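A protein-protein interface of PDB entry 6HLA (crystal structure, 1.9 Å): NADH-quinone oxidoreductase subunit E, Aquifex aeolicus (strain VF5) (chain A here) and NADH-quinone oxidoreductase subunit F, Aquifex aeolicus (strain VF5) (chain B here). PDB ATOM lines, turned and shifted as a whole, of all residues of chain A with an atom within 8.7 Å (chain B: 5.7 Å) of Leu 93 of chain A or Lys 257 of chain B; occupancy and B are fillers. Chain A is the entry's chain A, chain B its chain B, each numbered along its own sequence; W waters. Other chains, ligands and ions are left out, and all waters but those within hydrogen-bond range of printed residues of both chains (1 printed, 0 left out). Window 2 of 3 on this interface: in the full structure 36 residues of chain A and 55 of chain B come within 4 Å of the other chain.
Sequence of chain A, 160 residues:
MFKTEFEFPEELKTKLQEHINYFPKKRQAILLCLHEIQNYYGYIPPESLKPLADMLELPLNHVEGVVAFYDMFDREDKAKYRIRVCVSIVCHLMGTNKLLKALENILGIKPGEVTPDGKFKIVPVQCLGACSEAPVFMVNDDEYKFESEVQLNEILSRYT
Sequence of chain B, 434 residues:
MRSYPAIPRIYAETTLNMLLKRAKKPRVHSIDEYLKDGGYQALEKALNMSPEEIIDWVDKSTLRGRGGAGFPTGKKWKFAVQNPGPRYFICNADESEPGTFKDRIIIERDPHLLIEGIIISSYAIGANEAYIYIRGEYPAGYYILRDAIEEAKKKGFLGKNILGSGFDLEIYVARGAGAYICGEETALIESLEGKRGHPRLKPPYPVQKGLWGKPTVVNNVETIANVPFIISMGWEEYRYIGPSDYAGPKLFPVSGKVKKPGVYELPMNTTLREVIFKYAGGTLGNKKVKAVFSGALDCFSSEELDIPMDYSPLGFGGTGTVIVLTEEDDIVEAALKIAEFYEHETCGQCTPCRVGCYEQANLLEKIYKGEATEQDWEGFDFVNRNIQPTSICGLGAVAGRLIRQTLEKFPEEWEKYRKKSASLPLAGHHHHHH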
ATOM      1  N   CYS A  86     -13.191 -16.446 -10.318  1.00  0.00           N
ATOM      2  CA  CYS A  86     -11.954 -17.202 -10.194  1.00  0.00           C
ATOM      3  C   CYS A  86     -11.825 -17.788  -8.804  1.00  0.00           C
ATOM      4  O   CYS A  86     -11.914 -17.077  -7.805  1.00  0.00           O
ATOM      5  CB  CYS A  86     -10.737 -16.372 -10.569  1.00  0.00           C
ATOM      6  SG  CYS A  86      -9.188 -17.287 -10.437  1.00  0.00           S
ATOM      7  N   VAL A  87     -11.635 -19.096  -8.765  1.00  0.00           N
ATOM      8  CA  VAL A  87     -11.541 -19.868  -7.534  1.00  0.00           C
ATOM      9  C   VAL A  87     -10.114 -20.401  -7.330  1.00  0.00           C
ATOM     10  O   VAL A  87      -9.890 -21.214  -6.427  1.00  0.00           O
ATOM     11  CB  VAL A  87     -12.640 -20.975  -7.464  1.00  0.00           C
ATOM     12  CG1 VAL A  87     -14.049 -20.361  -7.432  1.00  0.00           C
ATOM     13  CG2 VAL A  87     -12.510 -21.983  -8.605  1.00  0.00           C
ATOM     14  N   SER A  88      -9.159 -19.943  -8.174  1.00  0.00           N
ATOM     15  CA  SER A  88      -7.758 -20.377  -8.076  1.00  0.00           C
ATOM     16  C   SER A  88      -6.996 -19.691  -6.964  1.00  0.00           C
ATOM     17  O   SER A  88      -7.526 -18.813  -6.292  1.00  0.00           O
ATOM     18  CB  SER A  88      -7.027 -20.267  -9.406  1.00  0.00           C
ATOM     19  OG  SER A  88      -7.523 -21.273 -10.264  1.00  0.00           O
ATOM     20  N   ILE A  89      -5.734 -20.095  -6.803  1.00  0.00           N
ATOM     21  CA  ILE A  89      -4.818 -19.776  -5.715  1.00  0.00           C
ATOM     22  C   ILE A  89      -4.714 -18.242  -5.333  1.00  0.00           C
ATOM     23  O   ILE A  89      -4.974 -17.911  -4.167  1.00  0.00           O
ATOM     24  CB  ILE A  89      -3.418 -20.444  -5.990  1.00  0.00           C
ATOM     25  CG1 ILE A  89      -2.400 -20.159  -4.868  1.00  0.00           C
ATOM     26  CG2 ILE A  89      -2.851 -20.102  -7.349  1.00  0.00           C
ATOM     27  CD1 ILE A  89      -2.638 -20.872  -3.578  1.00  0.00           C
ATOM     28  N   VAL A  90      -4.330 -17.336  -6.261  1.00  0.00           N
ATOM     29  CA  VAL A  90      -4.177 -15.913  -5.933  1.00  0.00           C
ATOM     30  C   VAL A  90      -5.509 -15.277  -5.500  1.00  0.00           C
ATOM     31  O   VAL A  90      -5.558 -14.580  -4.487  1.00  0.00           O
ATOM     32  CB  VAL A  90      -3.490 -15.058  -7.024  1.00  0.00           C
ATOM     33  CG1 VAL A  90      -3.006 -13.728  -6.426  1.00  0.00           C
ATOM     34  CG2 VAL A  90      -2.328 -15.811  -7.690  1.00  0.00           C
ATOM     35  N   CYS A  91      -6.580 -15.545  -6.242  1.00  0.00           N
ATOM     36  CA  CYS A  91      -7.880 -14.993  -5.896  1.00  0.00           C
ATOM     37  C   CYS A  91      -8.411 -15.519  -4.564  1.00  0.00           C
ATOM     38  O   CYS A  91      -8.900 -14.713  -3.776  1.00  0.00           O
ATOM     39  CB  CYS A  91      -8.850 -15.179  -7.043  1.00  0.00           C
ATOM     40  SG  CYS A  91      -8.395 -14.206  -8.495  1.00  0.00           S
ATOM     41  N   HIS A  92      -8.165 -16.816  -4.241  1.00  0.00           N
ATOM     42  CA  HIS A  92      -8.526 -17.398  -2.946  1.00  0.00           C
ATOM     43  C   HIS A  92      -7.808 -16.687  -1.776  1.00  0.00           C
ATOM     44  O   HIS A  92      -8.388 -16.490  -0.701  1.00  0.00           O
ATOM     45  CB  HIS A  92      -8.221 -18.913  -2.909  1.00  0.00           C
ATOM     46  CG  HIS A  92      -8.472 -19.497  -1.557  1.00  0.00           C
ATOM     47  ND1 HIS A  92      -9.764 -19.764  -1.118  1.00  0.00           N
ATOM     48  CD2 HIS A  92      -7.602 -19.759  -0.554  1.00  0.00           C
ATOM     49  CE1 HIS A  92      -9.631 -20.211   0.124  1.00  0.00           C
ATOM     50  NE2 HIS A  92      -8.347 -20.230   0.506  1.00  0.00           N
ATOM     51  N   LEU A  93      -6.541 -16.342  -2.007  1.00  0.00           N
ATOM     52  CA  LEU A  93      -5.653 -15.648  -1.093  1.00  0.00           C
ATOM     53  C   LEU A  93      -6.130 -14.207  -0.870  1.00  0.00           C
ATOM     54  O   LEU A  93      -6.038 -13.723   0.251  1.00  0.00           O
ATOM     55  CB  LEU A  93      -4.248 -15.627  -1.725  1.00  0.00           C
ATOM     56  CG  LEU A  93      -3.065 -16.283  -1.018  1.00  0.00           C
ATOM     57  CD1 LEU A  93      -3.344 -17.745  -0.664  1.00  0.00           C
ATOM     58  CD2 LEU A  93      -1.818 -16.174  -1.881  1.00  0.00           C
ATOM     59  N   MET A  94      -6.632 -13.532  -1.928  1.00  0.00           N
ATOM     60  CA  MET A  94      -7.069 -12.113  -1.872  1.00  0.00           C
ATOM     61  C   MET A  94      -8.577 -11.889  -1.630  1.00  0.00           C
ATOM     62  O   MET A  94      -8.972 -10.739  -1.413  1.00  0.00           O
ATOM     63  CB  MET A  94      -6.607 -11.302  -3.096  1.00  0.00           C
ATOM     64  CG  MET A  94      -5.091 -11.411  -3.419  1.00  0.00           C
ATOM     65  SD  MET A  94      -3.963 -11.190  -2.012  1.00  0.00           S
ATOM     66  CE  MET A  94      -4.219  -9.466  -1.646  1.00  0.00           C
ATOM     67  N   GLY A  95      -9.405 -12.935  -1.654  1.00  0.00           N
ATOM     68  CA  GLY A  95     -10.806 -12.707  -1.307  1.00  0.00           C
ATOM     69  C   GLY A  95     -11.945 -13.242  -2.138  1.00  0.00           C
ATOM     70  O   GLY A  95     -13.023 -12.646  -2.100  1.00  0.00           O
ATOM     71  N   THR A  96     -11.764 -14.405  -2.815  1.00  0.00           N
ATOM     72  CA  THR A  96     -12.830 -15.078  -3.582  1.00  0.00           C
ATOM     73  C   THR A  96     -14.080 -15.226  -2.705  1.00  0.00           C
ATOM     74  O   THR A  96     -15.185 -14.914  -3.154  1.00  0.00           O
ATOM     75  CB  THR A  96     -12.367 -16.474  -4.069  1.00  0.00           C
ATOM     76  OG1 THR A  96     -11.321 -16.331  -5.013  1.00  0.00           O
ATOM     77  CG2 THR A  96     -13.499 -17.296  -4.708  1.00  0.00           C
ATOM     78  N   ASN A  97     -13.897 -15.681  -1.450  1.00  0.00           N
ATOM     79  CA  ASN A  97     -15.006 -15.899  -0.526  1.00  0.00           C
ATOM     80  C   ASN A  97     -15.777 -14.613  -0.200  1.00  0.00           C
ATOM     81  O   ASN A  97     -17.003 -14.668  -0.079  1.00  0.00           O
ATOM     82  CB  ASN A  97     -14.540 -16.649   0.726  1.00  0.00           C
ATOM     83  CG  ASN A  97     -14.132 -18.095   0.448  1.00  0.00           C
ATOM     84  OD1 ASN A  97     -14.403 -18.677  -0.626  1.00  0.00           O
ATOM     85  ND2 ASN A  97     -13.459 -18.714   1.411  1.00  0.00           N
ATOM     86  N   LYS A  98     -15.080 -13.463  -0.130  1.00  0.00           N
ATOM     87  CA  LYS A  98     -15.691 -12.150   0.100  1.00  0.00           C
ATOM     88  C   LYS A  98     -16.521 -11.752  -1.125  1.00  0.00           C
ATOM     89  O   LYS A  98     -17.639 -11.263  -0.966  1.00  0.00           O
ATOM     90  CB  LYS A  98     -14.632 -11.077   0.432  1.00  0.00           C
ATOM     91  CG  LYS A  98     -13.908 -11.311   1.766  1.00  0.00           C
ATOM     92  CD  LYS A  98     -13.222 -10.041   2.280  1.00  0.00           C
ATOM     93  CE  LYS A  98     -11.797  -9.876   1.806  1.00  0.00           C
ATOM     94  NZ  LYS A  98     -10.844 -10.591   2.688  1.00  0.00           N
ATOM     95  N   CYS A 131      -4.331 -12.035 -11.987  1.00  0.00           N
ATOM     96  CA  CYS A 131      -4.002 -12.306 -10.587  1.00  0.00           C
ATOM     97  C   CYS A 131      -3.548 -11.075  -9.784  1.00  0.00           C
ATOM     98  O   CYS A 131      -3.868 -11.008  -8.603  1.00  0.00           O
ATOM     99  CB  CYS A 131      -2.993 -13.441 -10.515  1.00  0.00           C
ATOM    100  SG  CYS A 131      -3.260 -14.721 -11.780  1.00  0.00           S
ATOM    101  N   ALA A 134      -6.542  -9.639  -8.129  1.00  0.00           N
ATOM    102  CA  ALA A 134      -7.334 -10.586  -7.347  1.00  0.00           C
ATOM    103  C   ALA A 134      -8.152  -9.891  -6.208  1.00  0.00           C
ATOM    104  O   ALA A 134      -7.649  -8.939  -5.613  1.00  0.00           O
ATOM    105  CB  ALA A 134      -6.458 -11.677  -6.796  1.00  0.00           C
ATOM    106  N   PRO A 135      -9.402 -10.304  -5.910  1.00  0.00           N
ATOM    107  CA  PRO A 135     -10.169 -11.388  -6.544  1.00  0.00           C
ATOM    108  C   PRO A 135     -10.848 -10.925  -7.829  1.00  0.00           C
ATOM    109  O   PRO A 135     -11.549  -9.925  -7.846  1.00  0.00           O
ATOM    110  CB  PRO A 135     -11.109 -11.836  -5.424  1.00  0.00           C
ATOM    111  CG  PRO A 135     -11.352 -10.603  -4.606  1.00  0.00           C
ATOM    112  CD  PRO A 135     -10.180  -9.668  -4.824  1.00  0.00           C
ATOM    113  N   SER B 255       2.149 -11.366  -8.019  1.00  0.00           N
ATOM    114  CA  SER B 255       0.846 -11.273  -7.384  1.00  0.00           C
ATOM    115  C   SER B 255       0.879 -11.815  -5.967  1.00  0.00           C
ATOM    116  O   SER B 255       1.928 -12.227  -5.474  1.00  0.00           O
ATOM    117  CB  SER B 255      -0.213 -11.982  -8.226  1.00  0.00           C
ATOM    118  OG  SER B 255       0.040 -13.369  -8.293  1.00  0.00           O
ATOM    119  N   GLY B 256      -0.271 -11.753  -5.313  1.00  0.00           N
ATOM    120  CA  GLY B 256      -0.414 -12.175  -3.934  1.00  0.00           C
ATOM    121  C   GLY B 256      -0.207 -11.018  -2.981  1.00  0.00           C
ATOM    122  O   GLY B 256      -0.559  -9.862  -3.279  1.00  0.00           O
ATOM    123  N   LYS B 257       0.475 -11.325  -1.880  1.00  0.00           N
ATOM    124  CA  LYS B 257       0.703 -10.457  -0.735  1.00  0.00           C
ATOM    125  C   LYS B 257       1.856  -9.441  -0.912  1.00  0.00           C
ATOM    126  O   LYS B 257       2.688  -9.273  -0.021  1.00  0.00           O
ATOM    127  CB  LYS B 257       0.871 -11.330   0.519  1.00  0.00           C
ATOM    128  CG  LYS B 257      -0.303 -12.300   0.758  1.00  0.00           C
ATOM    129  CD  LYS B 257      -1.605 -11.577   1.155  1.00  0.00           C
ATOM    130  CE  LYS B 257      -2.699 -12.546   1.524  1.00  0.00           C
ATOM    131  NZ  LYS B 257      -2.564 -13.028   2.925  1.00  0.00           N
ATOM    132  N   VAL B 258       1.860  -8.733  -2.049  1.00  0.00           N
ATOM    133  CA  VAL B 258       2.825  -7.684  -2.358  1.00  0.00           C
ATOM    134  C   VAL B 258       2.108  -6.350  -2.386  1.00  0.00           C
ATOM    135  O   VAL B 258       0.906  -6.298  -2.673  1.00  0.00           O
ATOM    136  CB  VAL B 258       3.630  -7.915  -3.659  1.00  0.00           C
ATOM    137  CG1 VAL B 258       4.585  -9.086  -3.513  1.00  0.00           C
ATOM    138  CG2 VAL B 258       2.721  -8.085  -4.866  1.00  0.00           C
ATOM    139  N   LYS B 259       2.841  -5.270  -2.098  1.00  0.00           N
ATOM    140  CA  LYS B 259       2.258  -3.936  -2.108  1.00  0.00           C
ATOM    141  C   LYS B 259       1.908  -3.470  -3.534  1.00  0.00           C
ATOM    142  O   LYS B 259       0.864  -2.840  -3.741  1.00  0.00           O
ATOM    143  CB  LYS B 259       3.170  -2.930  -1.396  1.00  0.00           C
ATOM    144  CG  LYS B 259       3.185  -3.111   0.117  1.00  0.00           C
ATOM    145  CD  LYS B 259       3.833  -1.910   0.789  1.00  0.00           C
ATOM    146  CE  LYS B 259       4.359  -2.206   2.166  1.00  0.00           C
ATOM    147  NZ  LYS B 259       5.595  -3.030   2.115  1.00  0.00           N
ATOM    148  N   GLY B 282       7.725  -4.684  -1.582  1.00  0.00           N
ATOM    149  CA  GLY B 282       7.730  -5.505  -0.391  1.00  0.00           C
ATOM    150  C   GLY B 282       6.396  -6.156  -0.161  1.00  0.00           C
ATOM    151  O   GLY B 282       5.570  -6.248  -1.073  1.00  0.00           O
ATOM    152  N   THR B 283       6.169  -6.606   1.068  1.00  0.00           N
ATOM    153  CA  THR B 283       4.933  -7.334   1.381  1.00  0.00           C
ATOM    154  C   THR B 283       3.813  -6.447   1.912  1.00  0.00           C
ATOM    155  O   THR B 283       4.087  -5.408   2.508  1.00  0.00           O
ATOM    156  CB  THR B 283       5.223  -8.458   2.376  1.00  0.00           C
ATOM    157  OG1 THR B 283       5.794  -7.877   3.546  1.00  0.00           O
ATOM    158  CG2 THR B 283       6.157  -9.499   1.822  1.00  0.00           C
ATOM    159  N   LEU B 284       2.553  -6.899   1.753  1.00  0.00           N
ATOM    160  CA  LEU B 284       1.389  -6.213   2.314  1.00  0.00           C
ATOM    161  C   LEU B 284       1.481  -6.311   3.835  1.00  0.00           C
ATOM    162  O   LEU B 284       1.703  -7.406   4.368  1.00  0.00           O
ATOM    163  CB  LEU B 284       0.091  -6.892   1.860  1.00  0.00           C
ATOM    164  CG  LEU B 284      -0.406  -6.564   0.476  1.00  0.00           C
ATOM    165  CD1 LEU B 284      -1.579  -7.455   0.121  1.00  0.00           C
ATOM    166  CD2 LEU B 284      -0.797  -5.093   0.353  1.00  0.00           C
ATOM    167  N   ILE B 323       4.039 -15.619  -7.063  1.00  0.00           N
ATOM    168  CA  ILE B 323       2.874 -15.525  -6.189  1.00  0.00           C
ATOM    169  C   ILE B 323       3.444 -15.505  -4.779  1.00  0.00           C
ATOM    170  O   ILE B 323       4.082 -16.465  -4.370  1.00  0.00           O
ATOM    171  CB  ILE B 323       1.853 -16.671  -6.381  1.00  0.00           C
ATOM    172  CG1 ILE B 323       1.381 -16.781  -7.836  1.00  0.00           C
ATOM    173  CG2 ILE B 323       0.678 -16.509  -5.384  1.00  0.00           C
ATOM    174  CD1 ILE B 323       0.896 -18.225  -8.227  1.00  0.00           C
ATOM    175  N   VAL B 324       3.210 -14.416  -4.036  1.00  0.00           N
ATOM    176  CA  VAL B 324       3.778 -14.254  -2.705  1.00  0.00           C
ATOM    177  C   VAL B 324       2.780 -14.630  -1.618  1.00  0.00           C
ATOM    178  O   VAL B 324       1.638 -14.166  -1.619  1.00  0.00           O
ATOM    179  CB  VAL B 324       4.381 -12.836  -2.517  1.00  0.00           C
ATOM    180  CG1 VAL B 324       5.068 -12.716  -1.158  1.00  0.00           C
ATOM    181  CG2 VAL B 324       5.374 -12.519  -3.625  1.00  0.00           C
ATOM    182  N   LEU B 325       3.212 -15.498  -0.712  1.00  0.00           N
ATOM    183  CA  LEU B 325       2.429 -15.918   0.444  1.00  0.00           C
ATOM    184  C   LEU B 325       3.138 -15.394   1.670  1.00  0.00           C
ATOM    185  O   LEU B 325       4.375 -15.438   1.747  1.00  0.00           O
ATOM    186  CB  LEU B 325       2.281 -17.453   0.527  1.00  0.00           C
ATOM    187  CG  LEU B 325       1.263 -18.106  -0.417  1.00  0.00           C
ATOM    188  CD1 LEU B 325       1.861 -18.341  -1.797  1.00  0.00           C
ATOM    189  CD2 LEU B 325       0.816 -19.462   0.126  1.00  0.00           C
ATOM    190  N   THR B 326       2.378 -14.854   2.609  1.00  0.00           N
ATOM    191  CA  THR B 326       3.002 -14.351   3.825  1.00  0.00           C
ATOM    192  C   THR B 326       2.729 -15.304   5.001  1.00  0.00           C
ATOM    193  O   THR B 326       2.035 -16.314   4.840  1.00  0.00           O
ATOM    194  CB  THR B 326       2.687 -12.873   4.091  1.00  0.00           C
ATOM    195  OG1 THR B 326       1.283 -12.638   4.044  1.00  0.00           O
ATOM    196  CG2 THR B 326       3.415 -11.947   3.126  1.00  0.00           C
ATOM    197  N   GLU B 328       0.850 -15.555   7.542  1.00  0.00           N
ATOM    198  CA  GLU B 328      -0.522 -15.912   7.948  1.00  0.00           C
ATOM    199  C   GLU B 328      -1.261 -16.801   6.923  1.00  0.00           C
ATOM    200  O   GLU B 328      -2.383 -17.245   7.196  1.00  0.00           O
ATOM    201  CB  GLU B 328      -1.349 -14.637   8.317  1.00  0.00           C
ATOM    202  CG  GLU B 328      -2.229 -14.032   7.218  1.00  0.00           C
ATOM    203  CD  GLU B 328      -1.579 -13.062   6.251  1.00  0.00           C
ATOM    204  OE1 GLU B 328      -0.334 -13.082   6.122  1.00  0.00           O
ATOM    205  OE2 GLU B 328      -2.324 -12.274   5.623  1.00  0.00           O
ATOM    206  N   ASP B 329      -0.648 -17.045   5.751  1.00  0.00           N
ATOM    207  CA  ASP B 329      -1.244 -17.913   4.741  1.00  0.00           C
ATOM    208  C   ASP B 329      -0.973 -19.376   5.042  1.00  0.00           C
ATOM    209  O   ASP B 329       0.183 -19.780   5.125  1.00  0.00           O
ATOM    210  CB  ASP B 329      -0.799 -17.511   3.323  1.00  0.00           C
ATOM    211  CG  ASP B 329      -1.241 -16.101   2.956  1.00  0.00           C
ATOM    212  OD1 ASP B 329      -2.429 -15.770   3.183  1.00  0.00           O
ATOM    213  OD2 ASP B 329      -0.397 -15.326   2.460  1.00  0.00           O
ATOM    214  N   ALA B 334      -3.351 -23.528   0.712  1.00  0.00           N
ATOM    215  CA  ALA B 334      -2.761 -23.113  -0.574  1.00  0.00           C
ATOM    216  C   ALA B 334      -2.478 -24.341  -1.464  1.00  0.00           C
ATOM    217  O   ALA B 334      -2.742 -24.311  -2.673  1.00  0.00           O
ATOM    218  CB  ALA B 334      -1.474 -22.340  -0.334  1.00  0.00           C
HETATM  219  O   HOH W   1      -2.517 -10.301  -6.386  1.00  0.00           O
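Water W1 bridges O of Cys 131 of chain A (2.7 Å) and N of Gly 256 of chain B (2.9 Å).
Hydrophobic or aromatic side chains of chain B within 4 Å of the printed part of chain A: Leu 284, Ile 323, Leu 325 and Ala 334.
Hydrophobic or aromatic side chains of chain A that line the printed part of chain B: Ile 89, Val 90, Leu 93 and Met 94.
Among the printed residues, no Asp or Glu carboxylate lies within 4 Å of a Lys or Arg side-chain nitrogen of the other chain.
Lys 257 of chain B touches just these residues of chain A: Leu 93 (3.8 Å) and Met 94 (3.97 Å).
Gly 256 of chain B touches just these residues of chain A: Val 90 and Met 94.
Printed residues of chain B within 4 Å of Met 94 of chain A: Gly 256 (3.9 Å), Lys 257 (3.97 Å) and Leu 284 (3.8 Å).
Of the printed residues of chain B, Cys 131 of chain A touches Ser 255 (3.8 Å).
Of the printed residues of chain B, Val 90 of chain A touches Ser 255 (3.5 Å), Gly 256 (3.6 Å) and Ile 323 (3.8 Å).
The nearest printed residue of chain B that does not touch Leu 93 of chain A is Val 324 of chain B (4.01 Å).
The nearest residue of chain A that does not touch Lys 257 of chain B is Val 90 of chain A (6.2 Å).
The nearest printed residue of chain B that does not touch Cys 131 of chain A is Gly 256 of chain B (4.9 Å).
Ile 89 of chain A touches Ala 334 of chain B.
Ser 255 of chain B touches Val 90 of chain A.
N of Gly 256 of chain B touches CG1 of Val 90 of chain A (3.6 Å).
Val 90 of chain A touches Ile 323 of chain B.
Lys 257 of chain B touches Leu 93 of chain A (CE to O, 3.8 Å).
CG of Leu 325 of chain B touches CD2 of Leu 93 of chain A (3.9 Å).
SD of Met 94 of chain A touches O of Gly 256 of chain B, at 3.9 Å.
Met 94 of chain A touches Lys 257 of chain B.
Leu 284 of chain B touches Met 94 of chain A.
Cys 131 of chain A touches Ser 255 of chain B (CB to OG, 3.8 Å).
O of Ser 255 of chain B sits at hydrogen-bond distance from N of Val 324 of chain B, at 2.9 Å.
The backbone NH (N) of Leu 284 of chain B lies within hydrogen-bond range of the backbone carbonyl oxygen (O) of Lys 257 of chain B (3.0 Å).
O of Val 324 of chain B is in hydrogen-bond range of N of Lys 257 of chain B (3.1 Å).
The side-chain carboxylate (OE2) of Glu 328 of chain B lies within salt-bridge range of the side-chain amino group (NZ) of Lys 257 of chain B, at 2.8 Å.
The side-chain amino group (NZ) of Lys 257 of chain B lies within salt-bridge range of the side-chain carboxylate (OD1) of Asp 329 of chain B.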
